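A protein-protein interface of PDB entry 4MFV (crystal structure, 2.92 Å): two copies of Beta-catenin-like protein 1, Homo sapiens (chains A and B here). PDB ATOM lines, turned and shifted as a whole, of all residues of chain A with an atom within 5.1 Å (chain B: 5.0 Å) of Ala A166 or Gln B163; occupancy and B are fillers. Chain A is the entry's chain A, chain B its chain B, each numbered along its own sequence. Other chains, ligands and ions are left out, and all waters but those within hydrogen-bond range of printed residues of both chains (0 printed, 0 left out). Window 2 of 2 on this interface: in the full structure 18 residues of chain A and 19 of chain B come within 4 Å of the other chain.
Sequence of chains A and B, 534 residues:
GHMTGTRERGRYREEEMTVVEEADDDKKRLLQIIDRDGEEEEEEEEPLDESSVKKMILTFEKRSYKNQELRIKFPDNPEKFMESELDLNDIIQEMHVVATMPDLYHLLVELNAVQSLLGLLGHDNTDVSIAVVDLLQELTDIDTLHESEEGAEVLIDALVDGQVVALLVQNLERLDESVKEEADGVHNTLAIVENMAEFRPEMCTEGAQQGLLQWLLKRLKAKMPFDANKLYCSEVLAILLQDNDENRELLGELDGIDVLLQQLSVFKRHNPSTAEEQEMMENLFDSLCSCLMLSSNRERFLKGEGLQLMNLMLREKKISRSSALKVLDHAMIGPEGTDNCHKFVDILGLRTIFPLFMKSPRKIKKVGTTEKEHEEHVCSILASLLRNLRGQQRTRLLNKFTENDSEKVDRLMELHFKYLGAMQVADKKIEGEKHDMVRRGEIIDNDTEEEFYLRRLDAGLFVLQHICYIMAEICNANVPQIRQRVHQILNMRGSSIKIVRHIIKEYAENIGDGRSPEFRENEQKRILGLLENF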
ATOM      1  N   GLN A 163     -28.601 -17.237 -17.661  1.00  0.00           N
ATOM      2  CA  GLN A 163     -29.109 -15.875 -17.470  1.00  0.00           C
ATOM      3  C   GLN A 163     -29.834 -15.450 -18.733  1.00  0.00           C
ATOM      4  O   GLN A 163     -29.714 -14.332 -19.220  1.00  0.00           O
ATOM      5  CB  GLN A 163     -27.966 -14.922 -17.108  1.00  0.00           C
ATOM      6  CG  GLN A 163     -27.038 -15.467 -16.019  1.00  0.00           C
ATOM      7  CD  GLN A 163     -27.638 -15.357 -14.632  1.00  0.00           C
ATOM      8  OE1 GLN A 163     -28.043 -14.283 -14.208  1.00  0.00           O
ATOM      9  NE2 GLN A 163     -27.702 -16.464 -13.924  1.00  0.00           N
ATOM     10  N   VAL A 164     -30.661 -16.350 -19.225  1.00  0.00           N
ATOM     11  CA  VAL A 164     -31.249 -16.213 -20.537  1.00  0.00           C
ATOM     12  C   VAL A 164     -32.095 -14.959 -20.656  1.00  0.00           C
ATOM     13  O   VAL A 164     -32.047 -14.278 -21.667  1.00  0.00           O
ATOM     14  CB  VAL A 164     -32.079 -17.465 -20.858  1.00  0.00           C
ATOM     15  CG1 VAL A 164     -32.888 -17.871 -19.647  1.00  0.00           C
ATOM     16  CG2 VAL A 164     -32.963 -17.272 -22.075  1.00  0.00           C
ATOM     17  N   VAL A 165     -32.864 -14.643 -19.628  1.00  0.00           N
ATOM     18  CA  VAL A 165     -33.737 -13.487 -19.704  1.00  0.00           C
ATOM     19  C   VAL A 165     -32.931 -12.226 -19.877  1.00  0.00           C
ATOM     20  O   VAL A 165     -33.308 -11.339 -20.620  1.00  0.00           O
ATOM     21  CB  VAL A 165     -34.600 -13.332 -18.452  1.00  0.00           C
ATOM     22  CG1 VAL A 165     -35.530 -12.151 -18.619  1.00  0.00           C
ATOM     23  CG2 VAL A 165     -35.395 -14.595 -18.201  1.00  0.00           C
ATOM     24  N   ALA A 166     -31.815 -12.146 -19.174  1.00  0.00           N
ATOM     25  CA  ALA A 166     -30.987 -10.969 -19.257  1.00  0.00           C
ATOM     26  C   ALA A 166     -30.476 -10.813 -20.672  1.00  0.00           C
ATOM     27  O   ALA A 166     -30.492  -9.730 -21.232  1.00  0.00           O
ATOM     28  CB  ALA A 166     -29.832 -11.092 -18.290  1.00  0.00           C
ATOM     29  N   LEU A 167     -30.014 -11.897 -21.274  1.00  0.00           N
ATOM     30  CA  LEU A 167     -29.594 -11.843 -22.664  1.00  0.00           C
ATOM     31  C   LEU A 167     -30.773 -11.515 -23.563  1.00  0.00           C
ATOM     32  O   LEU A 167     -30.675 -10.721 -24.502  1.00  0.00           O
ATOM     33  CB  LEU A 167     -28.985 -13.175 -23.069  1.00  0.00           C
ATOM     34  CG  LEU A 167     -28.219 -13.869 -21.951  1.00  0.00           C
ATOM     35  CD1 LEU A 167     -27.392 -15.018 -22.484  1.00  0.00           C
ATOM     36  CD2 LEU A 167     -27.336 -12.864 -21.245  1.00  0.00           C
ATOM     37  N   LEU A 168     -31.901 -12.134 -23.257  1.00  0.00           N
ATOM     38  CA  LEU A 168     -33.100 -11.958 -24.043  1.00  0.00           C
ATOM     39  C   LEU A 168     -33.568 -10.531 -23.985  1.00  0.00           C
ATOM     40  O   LEU A 168     -33.985  -9.961 -24.978  1.00  0.00           O
ATOM     41  CB  LEU A 168     -34.193 -12.847 -23.491  1.00  0.00           C
ATOM     42  CG  LEU A 168     -34.294 -14.205 -24.153  1.00  0.00           C
ATOM     43  CD1 LEU A 168     -35.269 -15.053 -23.372  1.00  0.00           C
ATOM     44  CD2 LEU A 168     -34.766 -14.040 -25.579  1.00  0.00           C
ATOM     45  N   VAL A 169     -33.509  -9.957 -22.798  1.00  0.00           N
ATOM     46  CA  VAL A 169     -33.896  -8.577 -22.614  1.00  0.00           C
ATOM     47  C   VAL A 169     -32.979  -7.650 -23.379  1.00  0.00           C
ATOM     48  O   VAL A 169     -33.418  -6.660 -23.920  1.00  0.00           O
ATOM     49  CB  VAL A 169     -33.921  -8.195 -21.135  1.00  0.00           C
ATOM     50  CG1 VAL A 169     -34.213  -6.719 -20.979  1.00  0.00           C
ATOM     51  CG2 VAL A 169     -34.975  -9.009 -20.421  1.00  0.00           C
ATOM     52  N   GLN A 170     -31.694  -7.960 -23.397  1.00  0.00           N
ATOM     53  CA  GLN A 170     -30.758  -7.137 -24.134  1.00  0.00           C
ATOM     54  C   GLN A 170     -31.135  -7.174 -25.602  1.00  0.00           C
ATOM     55  O   GLN A 170     -31.127  -6.151 -26.280  1.00  0.00           O
ATOM     56  CB  GLN A 170     -29.330  -7.649 -23.951  1.00  0.00           C
ATOM     57  CG  GLN A 170     -28.564  -7.010 -22.804  1.00  0.00           C
ATOM     58  CD  GLN A 170     -27.405  -7.864 -22.333  1.00  0.00           C
ATOM     59  OE1 GLN A 170     -26.701  -8.462 -23.135  1.00  0.00           O
ATOM     60  NE2 GLN A 170     -27.203  -7.924 -21.026  1.00  0.00           N
ATOM     61  N   GLN A 210     -33.745  -9.353 -14.029  1.00  0.00           N
ATOM     62  CA  GLN A 210     -32.994  -9.179 -15.248  1.00  0.00           C
ATOM     63  C   GLN A 210     -33.468  -7.927 -15.947  1.00  0.00           C
ATOM     64  O   GLN A 210     -32.832  -7.457 -16.875  1.00  0.00           O
ATOM     65  CB  GLN A 210     -33.121 -10.396 -16.153  1.00  0.00           C
ATOM     66  CG  GLN A 210     -33.185 -11.717 -15.410  1.00  0.00           C
ATOM     67  CD  GLN A 210     -31.886 -12.500 -15.440  1.00  0.00           C
ATOM     68  OE1 GLN A 210     -30.806 -11.931 -15.341  1.00  0.00           O
ATOM     69  NE2 GLN A 210     -31.989 -13.817 -15.561  1.00  0.00           N
ATOM     70  N   LEU B 159     -18.290  -8.245 -19.275  1.00  0.00           N
ATOM     71  CA  LEU B 159     -18.348  -9.143 -18.131  1.00  0.00           C
ATOM     72  C   LEU B 159     -19.647  -9.029 -17.359  1.00  0.00           C
ATOM     73  O   LEU B 159     -20.204 -10.039 -16.908  1.00  0.00           O
ATOM     74  CB  LEU B 159     -17.184  -8.849 -17.182  1.00  0.00           C
ATOM     75  CG  LEU B 159     -15.839  -9.352 -17.695  1.00  0.00           C
ATOM     76  CD1 LEU B 159     -14.681  -8.736 -16.920  1.00  0.00           C
ATOM     77  CD2 LEU B 159     -15.798 -10.878 -17.643  1.00  0.00           C
ATOM     78  N   VAL B 160     -20.123  -7.803 -17.184  1.00  0.00           N
ATOM     79  CA  VAL B 160     -21.370  -7.600 -16.453  1.00  0.00           C
ATOM     80  C   VAL B 160     -22.571  -8.117 -17.264  1.00  0.00           C
ATOM     81  O   VAL B 160     -23.466  -8.771 -16.704  1.00  0.00           O
ATOM     82  CB  VAL B 160     -21.559  -6.132 -15.981  1.00  0.00           C
ATOM     83  CG1 VAL B 160     -21.616  -5.162 -17.144  1.00  0.00           C
ATOM     84  CG2 VAL B 160     -22.811  -5.989 -15.127  1.00  0.00           C
ATOM     85  N   ASP B 161     -22.561  -7.868 -18.577  1.00  0.00           N
ATOM     86  CA  ASP B 161     -23.571  -8.434 -19.480  1.00  0.00           C
ATOM     87  C   ASP B 161     -23.470  -9.949 -19.549  1.00  0.00           C
ATOM     88  O   ASP B 161     -24.475 -10.624 -19.695  1.00  0.00           O
ATOM     89  CB  ASP B 161     -23.446  -7.832 -20.871  1.00  0.00           C
ATOM     90  CG  ASP B 161     -23.889  -6.368 -20.912  1.00  0.00           C
ATOM     91  OD1 ASP B 161     -24.387  -5.879 -19.865  1.00  0.00           O
ATOM     92  OD2 ASP B 161     -23.743  -5.711 -21.981  1.00  0.00           O
ATOM     93  N   GLY B 162     -22.268 -10.479 -19.389  1.00  0.00           N
ATOM     94  CA  GLY B 162     -22.060 -11.921 -19.326  1.00  0.00           C
ATOM     95  C   GLY B 162     -22.436 -12.556 -18.014  1.00  0.00           C
ATOM     96  O   GLY B 162     -22.377 -13.783 -17.877  1.00  0.00           O
ATOM     97  N   GLN B 163     -22.805 -11.712 -17.049  1.00  0.00           N
ATOM     98  CA  GLN B 163     -23.324 -12.148 -15.750  1.00  0.00           C
ATOM     99  C   GLN B 163     -22.221 -12.914 -15.044  1.00  0.00           C
ATOM    100  O   GLN B 163     -22.399 -13.991 -14.495  1.00  0.00           O
ATOM    101  CB  GLN B 163     -24.617 -12.948 -15.920  1.00  0.00           C
ATOM    102  CG  GLN B 163     -25.593 -12.331 -16.935  1.00  0.00           C
ATOM    103  CD  GLN B 163     -26.496 -11.274 -16.343  1.00  0.00           C
ATOM    104  OE1 GLN B 163     -27.038 -11.439 -15.247  1.00  0.00           O
ATOM    105  NE2 GLN B 163     -26.676 -10.186 -17.068  1.00  0.00           N
ATOM    106  N   VAL B 164     -21.062 -12.291 -15.073  1.00  0.00           N
ATOM    107  CA  VAL B 164     -19.830 -12.872 -14.589  1.00  0.00           C
ATOM    108  C   VAL B 164     -19.887 -13.402 -13.157  1.00  0.00           C
ATOM    109  O   VAL B 164     -19.368 -14.476 -12.894  1.00  0.00           O
ATOM    110  CB  VAL B 164     -18.691 -11.844 -14.743  1.00  0.00           C
ATOM    111  CG1 VAL B 164     -19.050 -10.536 -14.065  1.00  0.00           C
ATOM    112  CG2 VAL B 164     -17.386 -12.380 -14.195  1.00  0.00           C
ATOM    113  N   VAL B 165     -20.513 -12.658 -12.244  1.00  0.00           N
ATOM    114  CA  VAL B 165     -20.606 -13.055 -10.812  1.00  0.00           C
ATOM    115  C   VAL B 165     -21.438 -14.321 -10.655  1.00  0.00           C
ATOM    116  O   VAL B 165     -21.020 -15.285  -9.999  1.00  0.00           O
ATOM    117  CB  VAL B 165     -21.273 -11.981  -9.917  1.00  0.00           C
ATOM    118  CG1 VAL B 165     -21.237 -12.421  -8.460  1.00  0.00           C
ATOM    119  CG2 VAL B 165     -20.602 -10.628 -10.073  1.00  0.00           C
ATOM    120  N   ALA B 166     -22.556 -14.396 -11.351  1.00  0.00           N
ATOM    121  CA  ALA B 166     -23.389 -15.565 -11.207  1.00  0.00           C
ATOM    122  C   ALA B 166     -22.628 -16.811 -11.622  1.00  0.00           C
ATOM    123  O   ALA B 166     -22.644 -17.817 -10.922  1.00  0.00           O
ATOM    124  CB  ALA B 166     -24.632 -15.403 -12.051  1.00  0.00           C
ATOM    125  N   LEU B 167     -21.929 -16.736 -12.743  1.00  0.00           N
ATOM    126  CA  LEU B 167     -21.098 -17.837 -13.187  1.00  0.00           C
ATOM    127  C   LEU B 167     -19.977 -18.061 -12.194  1.00  0.00           C
ATOM    128  O   LEU B 167     -19.633 -19.190 -11.839  1.00  0.00           O
ATOM    129  CB  LEU B 167     -20.525 -17.528 -14.559  1.00  0.00           C
ATOM    130  CG  LEU B 167     -21.474 -16.765 -15.475  1.00  0.00           C
ATOM    131  CD1 LEU B 167     -20.845 -16.528 -16.831  1.00  0.00           C
ATOM    132  CD2 LEU B 167     -22.768 -17.534 -15.621  1.00  0.00           C
ATOM    133  N   GLN B 210     -26.965 -11.911  -7.580  1.00  0.00           N
ATOM    134  CA  GLN B 210     -26.454 -13.141  -8.132  1.00  0.00           C
ATOM    135  C   GLN B 210     -26.247 -14.190  -7.057  1.00  0.00           C
ATOM    136  O   GLN B 210     -26.022 -15.345  -7.370  1.00  0.00           O
ATOM    137  CB  GLN B 210     -25.169 -12.898  -8.920  1.00  0.00           C
ATOM    138  CG  GLN B 210     -25.134 -11.578  -9.674  1.00  0.00           C
ATOM    139  CD  GLN B 210     -25.610 -11.681 -11.113  1.00  0.00           C
ATOM    140  OE1 GLN B 210     -26.765 -12.005 -11.375  1.00  0.00           O
ATOM    141  NE2 GLN B 210     -24.724 -11.379 -12.052  1.00  0.00           N
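The side-chain amide oxygen of Gln A163 lies close to the side-chain amide oxygen of Gln B163 (3.2 Å).
The backbone carbonyl oxygen (O) of Asp B161 sits close to the side-chain amide nitrogen (NE2) of Gln B163 (3.5 Å).
Among the printed residues, merely in contact across the chains: Gln A163 with Ala B166 (3.7 Å), Gln A163 with Gln B210 (3.9 Å), Ala A166 with Gln B163 (3.5 Å), Leu A167 with Asp B161 (3.95 Å), Gln A170 with Asp B161 (3.7 Å) and Gln A210 with Gln B163 (3.8 Å).
Ala A166 touches one residue of chain B. Of chain A, only Gln A163, Ala A166 and Gln A210 come within 4 Å of Gln B163. Of the printed residues of chain B, Gln A163 touches Gln B163, Ala B166 and Gln B210. Of the printed residues of chain A, Gln B210 touches Gln A163. Printed residues of chain A within 4 Å of Ala B166: Gln A163 (3.7 Å). Printed residues of chain A within 4 Å of Asp B161: Leu A167 (3.95 Å) and Gln A170 (3.7 Å). Printed residues of chain B within 4 Å of Leu A167: Asp B161 (3.95 Å). Val B160 touches none of the printed residues of chain A. Leu A168 touches none of the printed residues of chain B. The nearest printed residue of chain B that does not touch Ala A166 is Asp B161 (5.6 Å). The nearest residue of chain A that does not touch Gln B163 is Gln A170 (4.6 Å). The nearest printed residue of chain A that does not touch Asp B161 is Ala A166 (5.6 Å).
Hydrophobic or aromatic side chains of chain B that line the printed part of chain A: Ala B166. Along chain A the printed residues that touch a printed residue of chain B span positions 163 to 210. Among the printed residues, 7 pairs touch across the chains.
Gln B163 touches its own counterpart, Gln A163. Gln A163 touches Ala B166, and with the chains exchanged Ala A166 touches Gln B163. Gln A163 touches Gln B210, and with the chains exchanged Gln A210 touches Gln B163. Of the 7 pairs that touch across the chains among the printed residues, 5 have their exchanged pair printed and touching as well.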
